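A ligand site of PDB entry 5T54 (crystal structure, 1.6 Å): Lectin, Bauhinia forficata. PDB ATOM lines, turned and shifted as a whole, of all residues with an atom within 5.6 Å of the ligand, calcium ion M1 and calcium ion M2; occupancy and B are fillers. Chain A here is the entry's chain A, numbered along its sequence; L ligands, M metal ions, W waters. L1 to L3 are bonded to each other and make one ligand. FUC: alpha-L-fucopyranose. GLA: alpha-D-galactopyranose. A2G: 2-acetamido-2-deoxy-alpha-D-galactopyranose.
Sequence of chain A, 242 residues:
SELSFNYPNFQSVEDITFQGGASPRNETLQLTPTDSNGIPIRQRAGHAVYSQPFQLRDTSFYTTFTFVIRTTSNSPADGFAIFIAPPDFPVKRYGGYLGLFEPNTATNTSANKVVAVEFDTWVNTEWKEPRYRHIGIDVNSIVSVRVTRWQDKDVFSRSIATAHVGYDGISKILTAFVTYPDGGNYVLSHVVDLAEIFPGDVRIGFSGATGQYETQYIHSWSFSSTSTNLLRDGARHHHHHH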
ATOM      1  N   ARG A  42     -19.936  -9.770 -17.387  1.00  0.00           N
ATOM      2  CA  ARG A  42     -19.836  -8.418 -16.909  1.00  0.00           C
ATOM      3  C   ARG A  42     -20.203  -7.361 -17.953  1.00  0.00           C
ATOM      4  O   ARG A  42     -20.053  -7.561 -19.140  1.00  0.00           O
ATOM      5  CB  ARG A  42     -18.410  -8.151 -16.415  1.00  0.00           C
ATOM      6  CG  ARG A  42     -18.078  -8.923 -15.170  1.00  0.00           C
ATOM      7  CD  ARG A  42     -16.646  -8.552 -14.813  1.00  0.00           C
ATOM      8  NE  ARG A  42     -16.148  -9.489 -13.802  1.00  0.00           N
ATOM      9  CZ  ARG A  42     -16.012  -9.227 -12.508  1.00  0.00           C
ATOM     10  NH1 ARG A  42     -16.238  -8.001 -12.029  1.00  0.00           N
ATOM     11  NH2 ARG A  42     -15.592 -10.202 -11.719  1.00  0.00           N
ATOM     12  N   ALA A  77     -23.989  -6.848  -8.735  1.00  0.00           N
ATOM     13  CA  ALA A  77     -24.392  -5.625  -9.434  1.00  0.00           C
ATOM     14  C   ALA A  77     -25.020  -6.011 -10.726  1.00  0.00           C
ATOM     15  O   ALA A  77     -24.571  -6.988 -11.303  1.00  0.00           O
ATOM     16  CB  ALA A  77     -23.226  -4.730  -9.604  1.00  0.00           C
ATOM     17  N   ASP A  78     -26.040  -5.289 -11.237  1.00  0.00           N
ATOM     18  CA  ASP A  78     -26.543  -3.986 -10.752  1.00  0.00           C
ATOM     19  C   ASP A  78     -28.026  -3.988 -10.388  1.00  0.00           C
ATOM     20  O   ASP A  78     -28.505  -3.023  -9.732  1.00  0.00           O
ATOM     21  CB  ASP A  78     -26.284  -2.965 -11.837  1.00  0.00           C
ATOM     22  CG  ASP A  78     -24.873  -2.424 -11.750  1.00  0.00           C
ATOM     23  OD1 ASP A  78     -24.682  -1.474 -10.958  1.00  0.00           O
ATOM     24  OD2 ASP A  78     -23.978  -3.008 -12.480  1.00  0.00           O
ATOM     25  N   TYR A  94     -25.110  -0.528 -19.732  1.00  0.00           N
ATOM     26  CA  TYR A  94     -24.920  -1.540 -18.648  1.00  0.00           C
ATOM     27  C   TYR A  94     -24.422  -0.862 -17.358  1.00  0.00           C
ATOM     28  O   TYR A  94     -24.445   0.366 -17.232  1.00  0.00           O
ATOM     29  CB  TYR A  94     -23.979  -2.665 -19.137  1.00  0.00           C
ATOM     30  CG  TYR A  94     -22.766  -2.078 -19.773  1.00  0.00           C
ATOM     31  CD1 TYR A  94     -21.774  -1.399 -19.015  1.00  0.00           C
ATOM     32  CD2 TYR A  94     -22.632  -2.037 -21.152  1.00  0.00           C
ATOM     33  CE1 TYR A  94     -20.723  -0.740 -19.612  1.00  0.00           C
ATOM     34  CE2 TYR A  94     -21.508  -1.453 -21.723  1.00  0.00           C
ATOM     35  CZ  TYR A  94     -20.569  -0.734 -20.979  1.00  0.00           C
ATOM     36  OH  TYR A  94     -19.519  -0.052 -21.584  1.00  0.00           O
ATOM     37  N   GLY A  95     -24.127  -1.661 -16.334  1.00  0.00           N
ATOM     38  CA  GLY A  95     -23.737  -1.116 -15.028  1.00  0.00           C
ATOM     39  C   GLY A  95     -24.923  -0.473 -14.342  1.00  0.00           C
ATOM     40  O   GLY A  95     -26.073  -0.911 -14.477  1.00  0.00           O
ATOM     41  N   GLY A  96     -24.634   0.558 -13.578  1.00  0.00           N
ATOM     42  CA  GLY A  96     -25.622   1.214 -12.704  1.00  0.00           C
ATOM     43  C   GLY A  96     -26.744   1.898 -13.472  1.00  0.00           C
ATOM     44  O   GLY A  96     -27.752   2.263 -12.846  1.00  0.00           O
ATOM     45  N   TYR A  97     -26.543   2.147 -14.756  1.00  0.00           N
ATOM     46  CA  TYR A  97     -27.582   2.710 -15.608  1.00  0.00           C
ATOM     47  C   TYR A  97     -28.749   1.736 -15.829  1.00  0.00           C
ATOM     48  O   TYR A  97     -29.782   2.172 -16.424  1.00  0.00           O
ATOM     49  CB  TYR A  97     -27.002   3.212 -16.958  1.00  0.00           C
ATOM     50  CG  TYR A  97     -25.876   4.178 -16.697  1.00  0.00           C
ATOM     51  CD1 TYR A  97     -26.153   5.477 -16.250  1.00  0.00           C
ATOM     52  CD2 TYR A  97     -24.572   3.801 -16.810  1.00  0.00           C
ATOM     53  CE1 TYR A  97     -25.096   6.347 -15.918  1.00  0.00           C
ATOM     54  CE2 TYR A  97     -23.516   4.661 -16.457  1.00  0.00           C
ATOM     55  CZ  TYR A  97     -23.802   5.940 -16.041  1.00  0.00           C
ATOM     56  OH  TYR A  97     -22.816   6.839 -15.718  1.00  0.00           O
ATOM     57  N   LEU A  98     -28.622   0.442 -15.458  1.00  0.00           N
ATOM     58  CA  LEU A  98     -29.699  -0.573 -15.508  1.00  0.00           C
ATOM     59  C   LEU A  98     -30.294  -0.786 -16.866  1.00  0.00           C
ATOM     60  O   LEU A  98     -31.429  -1.256 -17.008  1.00  0.00           O
ATOM     61  CB  LEU A  98     -30.820  -0.143 -14.485  1.00  0.00           C
ATOM     62  CG  LEU A  98     -30.355  -0.197 -13.044  1.00  0.00           C
ATOM     63  CD1 LEU A  98     -31.443   0.290 -12.097  1.00  0.00           C
ATOM     64  CD2 LEU A  98     -29.895  -1.576 -12.675  1.00  0.00           C
ATOM     65  N   GLU A 118     -37.396   0.109 -10.073  1.00  0.00           N
ATOM     66  CA  GLU A 118     -36.085  -0.528 -10.023  1.00  0.00           C
ATOM     67  C   GLU A 118     -35.829  -1.337  -8.762  1.00  0.00           C
ATOM     68  O   GLU A 118     -36.326  -1.004  -7.670  1.00  0.00           O
ATOM     69  CB  GLU A 118     -34.956   0.524 -10.222  1.00  0.00           C
ATOM     70  CG  GLU A 118     -34.819   1.567  -9.159  1.00  0.00           C
ATOM     71  CD  GLU A 118     -33.492   2.305  -9.250  1.00  0.00           C
ATOM     72  OE1 GLU A 118     -33.242   2.931 -10.316  1.00  0.00           O
ATOM     73  OE2 GLU A 118     -32.761   2.421  -8.237  1.00  0.00           O
ATOM     74  N   ASP A 120     -32.430  -2.370  -7.039  1.00  0.00           N
ATOM     75  CA  ASP A 120     -31.053  -1.883  -7.228  1.00  0.00           C
ATOM     76  C   ASP A 120     -30.134  -2.576  -6.211  1.00  0.00           C
ATOM     77  O   ASP A 120     -30.244  -2.386  -4.994  1.00  0.00           O
ATOM     78  CB  ASP A 120     -31.031  -0.370  -7.109  1.00  0.00           C
ATOM     79  CG  ASP A 120     -29.722   0.214  -7.469  1.00  0.00           C
ATOM     80  OD1 ASP A 120     -28.704  -0.493  -7.340  1.00  0.00           O
ATOM     81  OD2 ASP A 120     -29.654   1.429  -7.876  1.00  0.00           O
ATOM     82  N   THR A 121     -29.216  -3.447  -6.714  1.00  0.00           N
ATOM     83  CA  THR A 121     -28.369  -4.260  -5.896  1.00  0.00           C
ATOM     84  C   THR A 121     -27.007  -3.647  -5.635  1.00  0.00           C
ATOM     85  O   THR A 121     -26.260  -4.257  -4.867  1.00  0.00           O
ATOM     86  CB  THR A 121     -28.127  -5.642  -6.528  1.00  0.00           C
ATOM     87  OG1 THR A 121     -27.532  -5.469  -7.870  1.00  0.00           O
ATOM     88  CG2 THR A 121     -29.427  -6.464  -6.617  1.00  0.00           C
ATOM     89  N   TRP A 122     -26.655  -2.562  -6.313  1.00  0.00           N
ATOM     90  CA  TRP A 122     -25.298  -1.989  -6.189  1.00  0.00           C
ATOM     91  C   TRP A 122     -25.415  -0.512  -5.871  1.00  0.00           C
ATOM     92  O   TRP A 122     -25.959   0.255  -6.709  1.00  0.00           O
ATOM     93  CB  TRP A 122     -24.504  -2.180  -7.480  1.00  0.00           C
ATOM     94  CG  TRP A 122     -23.136  -1.561  -7.447  1.00  0.00           C
ATOM     95  CD1 TRP A 122     -22.900  -0.284  -7.737  1.00  0.00           C
ATOM     96  CD2 TRP A 122     -21.872  -2.153  -7.091  1.00  0.00           C
ATOM     97  NE1 TRP A 122     -21.553   0.009  -7.583  1.00  0.00           N
ATOM     98  CE2 TRP A 122     -20.909  -1.140  -7.209  1.00  0.00           C
ATOM     99  CE3 TRP A 122     -21.486  -3.439  -6.632  1.00  0.00           C
ATOM    100  CZ2 TRP A 122     -19.539  -1.350  -6.961  1.00  0.00           C
ATOM    101  CZ3 TRP A 122     -20.119  -3.683  -6.407  1.00  0.00           C
ATOM    102  CH2 TRP A 122     -19.172  -2.639  -6.559  1.00  0.00           C
ATOM    103  N   VAL A 123     -24.905  -0.113  -4.713  1.00  0.00           N
ATOM    104  CA  VAL A 123     -24.858   1.274  -4.353  1.00  0.00           C
ATOM    105  C   VAL A 123     -23.829   2.090  -5.241  1.00  0.00           C
ATOM    106  O   VAL A 123     -22.627   1.885  -5.156  1.00  0.00           O
ATOM    107  CB  VAL A 123     -24.541   1.468  -2.852  1.00  0.00           C
ATOM    108  CG1 VAL A 123     -24.319   2.916  -2.510  1.00  0.00           C
ATOM    109  CG2 VAL A 123     -25.630   0.822  -2.015  1.00  0.00           C
ATOM    110  N   ASN A 124     -24.368   3.003  -6.067  1.00  0.00           N
ATOM    111  CA  ASN A 124     -23.588   3.872  -6.887  1.00  0.00           C
ATOM    112  C   ASN A 124     -23.339   5.219  -6.229  1.00  0.00           C
ATOM    113  O   ASN A 124     -24.208   5.807  -5.578  1.00  0.00           O
ATOM    114  CB  ASN A 124     -24.290   4.113  -8.207  1.00  0.00           C
ATOM    115  CG  ASN A 124     -24.273   2.903  -9.077  1.00  0.00           C
ATOM    116  OD1 ASN A 124     -25.239   2.171  -9.109  1.00  0.00           O
ATOM    117  ND2 ASN A 124     -23.218   2.731  -9.874  1.00  0.00           N
ATOM    118  N   THR A 125     -22.105   5.697  -6.361  1.00  0.00           N
ATOM    119  CA  THR A 125     -21.740   7.002  -5.904  1.00  0.00           C
ATOM    120  C   THR A 125     -21.573   8.015  -7.039  1.00  0.00           C
ATOM    121  O   THR A 125     -21.374   9.206  -6.787  1.00  0.00           O
ATOM    122  CB  THR A 125     -20.434   7.001  -5.061  1.00  0.00           C
ATOM    123  OG1 THR A 125     -19.392   6.357  -5.782  1.00  0.00           O
ATOM    124  CG2 THR A 125     -20.669   6.326  -3.701  1.00  0.00           C
ATOM    125  N   GLU A 126     -21.703   7.557  -8.291  1.00  0.00           N
ATOM    126  CA  GLU A 126     -21.631   8.393  -9.437  1.00  0.00           C
ATOM    127  C   GLU A 126     -22.837   9.355  -9.609  1.00  0.00           C
ATOM    128  O   GLU A 126     -22.741  10.301 -10.421  1.00  0.00           O
ATOM    129  CB  GLU A 126     -21.445   7.524 -10.714  1.00  0.00           C
ATOM    130  CG  GLU A 126     -20.223   6.545 -10.693  1.00  0.00           C
ATOM    131  CD  GLU A 126     -20.427   5.187 -10.108  1.00  0.00           C
ATOM    132  OE1 GLU A 126     -21.372   4.984  -9.332  1.00  0.00           O
ATOM    133  OE2 GLU A 126     -19.610   4.287 -10.493  1.00  0.00           O
ATOM    134  N   TRP A 127     -23.918   9.087  -8.917  1.00  0.00           N
ATOM    135  CA  TRP A 127     -25.111   9.964  -8.810  1.00  0.00           C
ATOM    136  C   TRP A 127     -25.675   9.697  -7.423  1.00  0.00           C
ATOM    137  O   TRP A 127     -25.227   8.760  -6.689  1.00  0.00           O
ATOM    138  CB  TRP A 127     -26.195   9.597  -9.868  1.00  0.00           C
ATOM    139  CG  TRP A 127     -26.469   8.125  -9.949  1.00  0.00           C
ATOM    140  CD1 TRP A 127     -27.390   7.366  -9.208  1.00  0.00           C
ATOM    141  CD2 TRP A 127     -25.872   7.205 -10.850  1.00  0.00           C
ATOM    142  NE1 TRP A 127     -27.328   6.054  -9.590  1.00  0.00           N
ATOM    143  CE2 TRP A 127     -26.426   5.945 -10.611  1.00  0.00           C
ATOM    144  CE3 TRP A 127     -24.886   7.337 -11.861  1.00  0.00           C
ATOM    145  CZ2 TRP A 127     -26.064   4.835 -11.333  1.00  0.00           C
ATOM    146  CZ3 TRP A 127     -24.533   6.176 -12.554  1.00  0.00           C
ATOM    147  CH2 TRP A 127     -25.110   4.975 -12.304  1.00  0.00           C
ATOM    148  N   GLU A 129     -27.875   8.268  -4.719  1.00  0.00           N
ATOM    149  CA  GLU A 129     -28.857   7.224  -4.330  1.00  0.00           C
ATOM    150  C   GLU A 129     -28.513   6.741  -2.938  1.00  0.00           C
ATOM    151  O   GLU A 129     -27.438   7.189  -2.368  1.00  0.00           O
ATOM    152  CB  GLU A 129     -28.951   6.068  -5.352  1.00  0.00           C
ATOM    153  CG  GLU A 129     -27.682   5.245  -5.547  1.00  0.00           C
ATOM    154  CD  GLU A 129     -27.856   4.184  -6.696  1.00  0.00           C
ATOM    155  OE1 GLU A 129     -28.755   4.356  -7.557  1.00  0.00           O
ATOM    156  OE2 GLU A 129     -27.177   3.134  -6.665  1.00  0.00           O
ATOM    157  N   PRO A 130     -29.413   5.998  -2.315  1.00  0.00           N
ATOM    158  CA  PRO A 130     -29.151   5.632  -0.901  1.00  0.00           C
ATOM    159  C   PRO A 130     -27.922   4.785  -0.715  1.00  0.00           C
ATOM    160  O   PRO A 130     -27.461   4.102  -1.652  1.00  0.00           O
ATOM    161  CB  PRO A 130     -30.391   4.816  -0.498  1.00  0.00           C
ATOM    162  CG  PRO A 130     -31.410   5.140  -1.490  1.00  0.00           C
ATOM    163  CD  PRO A 130     -30.686   5.439  -2.771  1.00  0.00           C
ATOM    164  N   HIS A 134     -31.784  -0.982  -2.562  1.00  0.00           N
ATOM    165  CA  HIS A 134     -33.003  -0.231  -2.531  1.00  0.00           C
ATOM    166  C   HIS A 134     -33.885  -0.592  -3.683  1.00  0.00           C
ATOM    167  O   HIS A 134     -33.445  -1.028  -4.728  1.00  0.00           O
ATOM    168  CB  HIS A 134     -32.745   1.306  -2.471  1.00  0.00           C
ATOM    169  CG  HIS A 134     -31.845   1.826  -3.560  1.00  0.00           C
ATOM    170  ND1 HIS A 134     -30.470   1.802  -3.452  1.00  0.00           N
ATOM    171  CD2 HIS A 134     -32.119   2.350  -4.770  1.00  0.00           C
ATOM    172  CE1 HIS A 134     -29.946   2.304  -4.560  1.00  0.00           C
ATOM    173  NE2 HIS A 134     -30.936   2.670  -5.348  1.00  0.00           N
ATOM    174  N   ILE A 142     -32.133   8.279 -13.445  1.00  0.00           N
ATOM    175  CA  ILE A 142     -31.592   7.214 -12.633  1.00  0.00           C
ATOM    176  C   ILE A 142     -31.625   7.562 -11.121  1.00  0.00           C
ATOM    177  O   ILE A 142     -31.410   6.693 -10.300  1.00  0.00           O
ATOM    178  CB  ILE A 142     -30.170   6.862 -13.147  1.00  0.00           C
ATOM    179  CG1 ILE A 142     -29.702   5.470 -12.729  1.00  0.00           C
ATOM    180  CG2 ILE A 142     -29.161   7.936 -12.732  1.00  0.00           C
ATOM    181  CD1 ILE A 142     -30.533   4.296 -13.116  1.00  0.00           C
ATOM    182  N   SER A 144     -33.834   8.137  -8.278  1.00  0.00           N
ATOM    183  CA  SER A 144     -35.237   7.715  -8.024  1.00  0.00           C
ATOM    184  C   SER A 144     -36.005   8.858  -7.319  1.00  0.00           C
ATOM    185  O   SER A 144     -35.444   9.579  -6.487  1.00  0.00           O
ATOM    186  CB  SER A 144     -35.294   6.512  -7.101  1.00  0.00           C
ATOM    187  OG  SER A 144     -34.611   5.391  -7.658  1.00  0.00           O
ATOM    188  N   THR A 210     -25.631  -5.915 -15.681  1.00  0.00           N
ATOM    189  CA  THR A 210     -24.424  -6.141 -14.925  1.00  0.00           C
ATOM    190  C   THR A 210     -23.393  -5.064 -15.252  1.00  0.00           C
ATOM    191  O   THR A 210     -23.478  -4.444 -16.305  1.00  0.00           O
ATOM    192  CB  THR A 210     -23.812  -7.566 -15.253  1.00  0.00           C
ATOM    193  OG1 THR A 210     -23.530  -7.588 -16.655  1.00  0.00           O
ATOM    194  CG2 THR A 210     -24.721  -8.699 -14.890  1.00  0.00           C
ATOM    195  N   GLY A 211     -22.312  -4.884 -14.469  1.00  0.00           N
ATOM    196  CA  GLY A 211     -22.174  -5.461 -13.136  1.00  0.00           C
ATOM    197  C   GLY A 211     -21.341  -6.710 -13.048  1.00  0.00           C
ATOM    198  O   GLY A 211     -20.378  -6.931 -13.815  1.00  0.00           O
ATOM    199  N   GLN A 212     -21.677  -7.499 -12.067  1.00  0.00           N
ATOM    200  CA  GLN A 212     -20.903  -8.667 -11.740  1.00  0.00           C
ATOM    201  C   GLN A 212     -21.702  -9.635 -10.831  1.00  0.00           C
ATOM    202  O   GLN A 212     -22.464  -9.177  -9.981  1.00  0.00           O
ATOM    203  CB  GLN A 212     -19.593  -8.263 -11.027  1.00  0.00           C
ATOM    204  CG  GLN A 212     -19.810  -7.479  -9.729  1.00  0.00           C
ATOM    205  CD  GLN A 212     -18.553  -7.014  -9.070  1.00  0.00           C
ATOM    206  OE1 GLN A 212     -17.519  -6.889  -9.721  1.00  0.00           O
ATOM    207  NE2 GLN A 212     -18.578  -6.900  -7.747  1.00  0.00           N
HETATM  208  C1  FUC L   1     -17.881   3.060  -7.992  1.00  0.00           C
HETATM  209  C2  FUC L   1     -19.167   3.248  -7.196  1.00  0.00           C
HETATM  210  C3  FUC L   1     -19.075   2.643  -5.802  1.00  0.00           C
HETATM  211  C4  FUC L   1     -17.799   3.114  -5.054  1.00  0.00           C
HETATM  212  C5  FUC L   1     -16.654   2.825  -5.998  1.00  0.00           C
HETATM  213  C6  FUC L   1     -15.290   3.126  -5.340  1.00  0.00           C
HETATM  214  O2  FUC L   1     -20.268   2.733  -7.994  1.00  0.00           O
HETATM  215  O3  FUC L   1     -20.205   3.117  -5.083  1.00  0.00           O
HETATM  216  O4  FUC L   1     -17.982   4.479  -4.739  1.00  0.00           O
HETATM  217  O5  FUC L   1     -16.813   3.595  -7.184  1.00  0.00           O
HETATM  218  C1  GLA L   2     -15.343   1.391  -8.996  1.00  0.00           C
HETATM  219  C2  GLA L   2     -16.744   1.664  -9.459  1.00  0.00           C
HETATM  220  C3  GLA L   2     -17.194   0.565 -10.384  1.00  0.00           C
HETATM  221  C4  GLA L   2     -16.158   0.296 -11.444  1.00  0.00           C
HETATM  222  C5  GLA L   2     -14.771   0.047 -10.913  1.00  0.00           C
HETATM  223  C6  GLA L   2     -13.750  -0.034 -12.066  1.00  0.00           C
HETATM  224  O1  GLA L   2     -15.402   0.228  -8.193  1.00  0.00           O
HETATM  225  O2  GLA L   2     -17.672   1.689  -8.366  1.00  0.00           O
HETATM  226  O3  GLA L   2     -18.511   0.865 -10.939  1.00  0.00           O
HETATM  227  O4  GLA L   2     -16.140   1.461 -12.226  1.00  0.00           O
HETATM  228  O5  GLA L   2     -14.429   1.179 -10.092  1.00  0.00           O
HETATM  229  O6  GLA L   2     -12.547  -0.469 -11.390  1.00  0.00           O
HETATM  230  O5  A2G L   3     -18.931  -1.314 -11.740  1.00  0.00           O
HETATM  231  C1  A2G L   3     -19.069   0.086 -11.963  1.00  0.00           C
HETATM  232  C2  A2G L   3     -20.519   0.517 -12.150  1.00  0.00           C
HETATM  233  N2  A2G L   3     -20.541   1.935 -12.339  1.00  0.00           N
HETATM  234  C3  A2G L   3     -21.351   0.007 -11.015  1.00  0.00           C
HETATM  235  O3  A2G L   3     -22.713   0.347 -11.327  1.00  0.00           O
HETATM  236  C4  A2G L   3     -21.125  -1.505 -10.877  1.00  0.00           C
HETATM  237  O4  A2G L   3     -21.541  -2.290 -12.011  1.00  0.00           O
HETATM  238  C5  A2G L   3     -19.644  -1.752 -10.588  1.00  0.00           C
HETATM  239  C6  A2G L   3     -19.346  -3.234 -10.393  1.00  0.00           C
HETATM  240  O6  A2G L   3     -17.931  -3.362 -10.077  1.00  0.00           O
HETATM  241  C7  A2G L   3     -21.334   2.506 -13.223  1.00  0.00           C
HETATM  242  O7  A2G L   3     -22.034   1.845 -14.002  1.00  0.00           O
HETATM  243  C8  A2G L   3     -21.397   4.015 -13.217  1.00  0.00           C
HETATM  244 CA    CA M   1     -27.268   1.388  -8.301  1.00  0.00          CA
HETATM  245 CA    CA M   2     -30.844   3.314  -7.648  1.00  0.00          CA
HETATM  246  O   HOH W   1     -30.831   3.976  -9.811  1.00  0.00           O
HETATM  247  O   HOH W   2     -17.565   4.433 -12.213  1.00  0.00           O
HETATM  248  O   HOH W   3     -28.236   2.587 -10.193  1.00  0.00           O
HETATM  249  O   HOH W   4     -13.101   0.055  -6.337  1.00  0.00           O
HETATM  250  O   HOH W   5     -21.785   1.431 -16.738  1.00  0.00           O
HETATM  251  O   HOH W   6     -16.310  -2.556  -8.310  1.00  0.00           O
HETATM  252  O   HOH W   7     -26.876  -0.507  -9.764  1.00  0.00           O
HETATM  253  O   HOH W   8     -20.460   2.995  -2.321  1.00  0.00           O
HETATM  254  O   HOH W   9     -20.394  -2.653 -14.425  1.00  0.00           O
HETATM  255  O   HOH W  10     -15.813  -3.140 -11.975  1.00  0.00           O
HETATM  256  O   HOH W  11     -32.131   5.096  -6.958  1.00  0.00           O
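An oxygen (O4) of A2G L3 sits at hydrogen-bond distance from the side-chain carboxylate of Asp 78 (2.6 Å). ND2 of Asn 124 is in hydrogen-bond range of O3 of A2G L3. O4 of FUC L1 sits at hydrogen-bond distance from OG1 of Thr 125. O7 of A2G L3 is in hydrogen-bond range of N of Gly 96 (2.9 Å). An oxygen (O2) of FUC L1 sits at hydrogen-bond distance from the side-chain carboxylate (OE1) of Glu 126, at 2.8 Å. An oxygen (O3) of FUC L1 lies within hydrogen-bond range of the backbone NH (N) of Thr 125 (3.4 Å). The indole nitrogen of Trp 122 sits at hydrogen-bond distance from an oxygen (O2) of FUC L1. An oxygen (O3) of FUC L1 sits at hydrogen-bond distance from the backbone carbonyl oxygen of Val 123 (2.7 Å).
The side-chain amide nitrogen (ND2) of Asn 124 sits at hydrogen-bond distance from the side-chain carboxylate (OE1) of Glu 126 (3.0 Å). The side-chain carboxylate (OE1) of Glu 129 sits close to the indole nitrogen (NE1) of Trp 127 (3.0 Å). The side-chain carboxylate (OD2) of Asp 78 lies close to the backbone NH (N) of Gly 211 (3.2 Å). The backbone NH (N) of Gly 95 is in hydrogen-bond range of the backbone carbonyl oxygen (O) of Thr 210 (2.9 Å). N of Thr 121 is in hydrogen-bond range of O of Asp 78 (3.1 Å). The backbone carbonyl oxygen (O) of Ala 77 lies within hydrogen-bond range of the backbone NH (N) of Gln 212. The guanidinium group of Arg 42 lies within hydrogen-bond range of the side-chain amide oxygen of Gln 212 (2.9 Å). The backbone NH of Gly 96 lies within hydrogen-bond range of the side-chain carboxylate of Asp 78 (3.3 Å).
CB of Ala 77 touches O4 of A2G L3, 3.8 Å away. CA of Gly 95 touches O7 of A2G L3 (3.6 Å). CE2 of Tyr 97 touches C8 of A2G L3, at 3.9 Å. Trp 127 touches the ligand. CA of Gly 211 touches O4 of A2G L3 (3.4 Å). OE1 of Gln 212 touches O6 of A2G L3 (3.6 Å). Hydrophobic or aromatic side chains that line the ligand: Ala 77, Tyr 97, Trp 122 and Trp 127. Of the 25 residues printed, 13 come within 4 Å of the ligand. Along chain A the residues within 4 Å of the ligand span positions 77 to 212. The nearest printed residue that does not touch the ligand is Tyr 94 (4.3 Å).
Four residues have an atom within 4 Å of calcium ion M1: Asp 120, Trp 122, Asn 124 and Glu 129. The nearest printed residue that does not touch calcium ion M1 is Val 123 (4.6 Å).
Calcium ion M1 is bound by the side-chain amide oxygen (OD1) of Asn 124 (2.3 Å), the backbone carbonyl oxygen (O) of Trp 122 (2.4 Å), the side-chain carboxylate (OE2) of Glu 129 (2.4 Å), the side-chain carboxylate (OD2) of Asp 120 (2.4 Å), water W7 (2.4 Å), water W3 (2.4 Å) and the side-chain carboxylate (OD1) of Asp 120 (2.6 Å). Calcium ion M1 has seven donor atoms within binding distance.
Calcium ion M2 is bound by OE2 of Glu 118 (2.2 Å), OD2 of Asp 120 (2.2 Å), water W1 (2.3 Å), water W11 (2.3 Å), OE1 of Glu 129 (2.3 Å) and NE2 of His 134 (2.4 Å). Calcium ion M2 has six donor atoms within binding distance.
Water W1 lies within hydrogen-bond range of OE1 of Glu 118 and O of Ile 142. Water W9 bridges O4 of A2G L3 and N of Gly 211. Water W5 lies within hydrogen-bond range of O7 of A2G L3 (2.8 Å) and O of Tyr 94 (2.9 Å). Water W2 lies within hydrogen-bond range of OE2 of Glu 126 (2.7 Å) and O4 of GLA L2 (3.3 Å).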
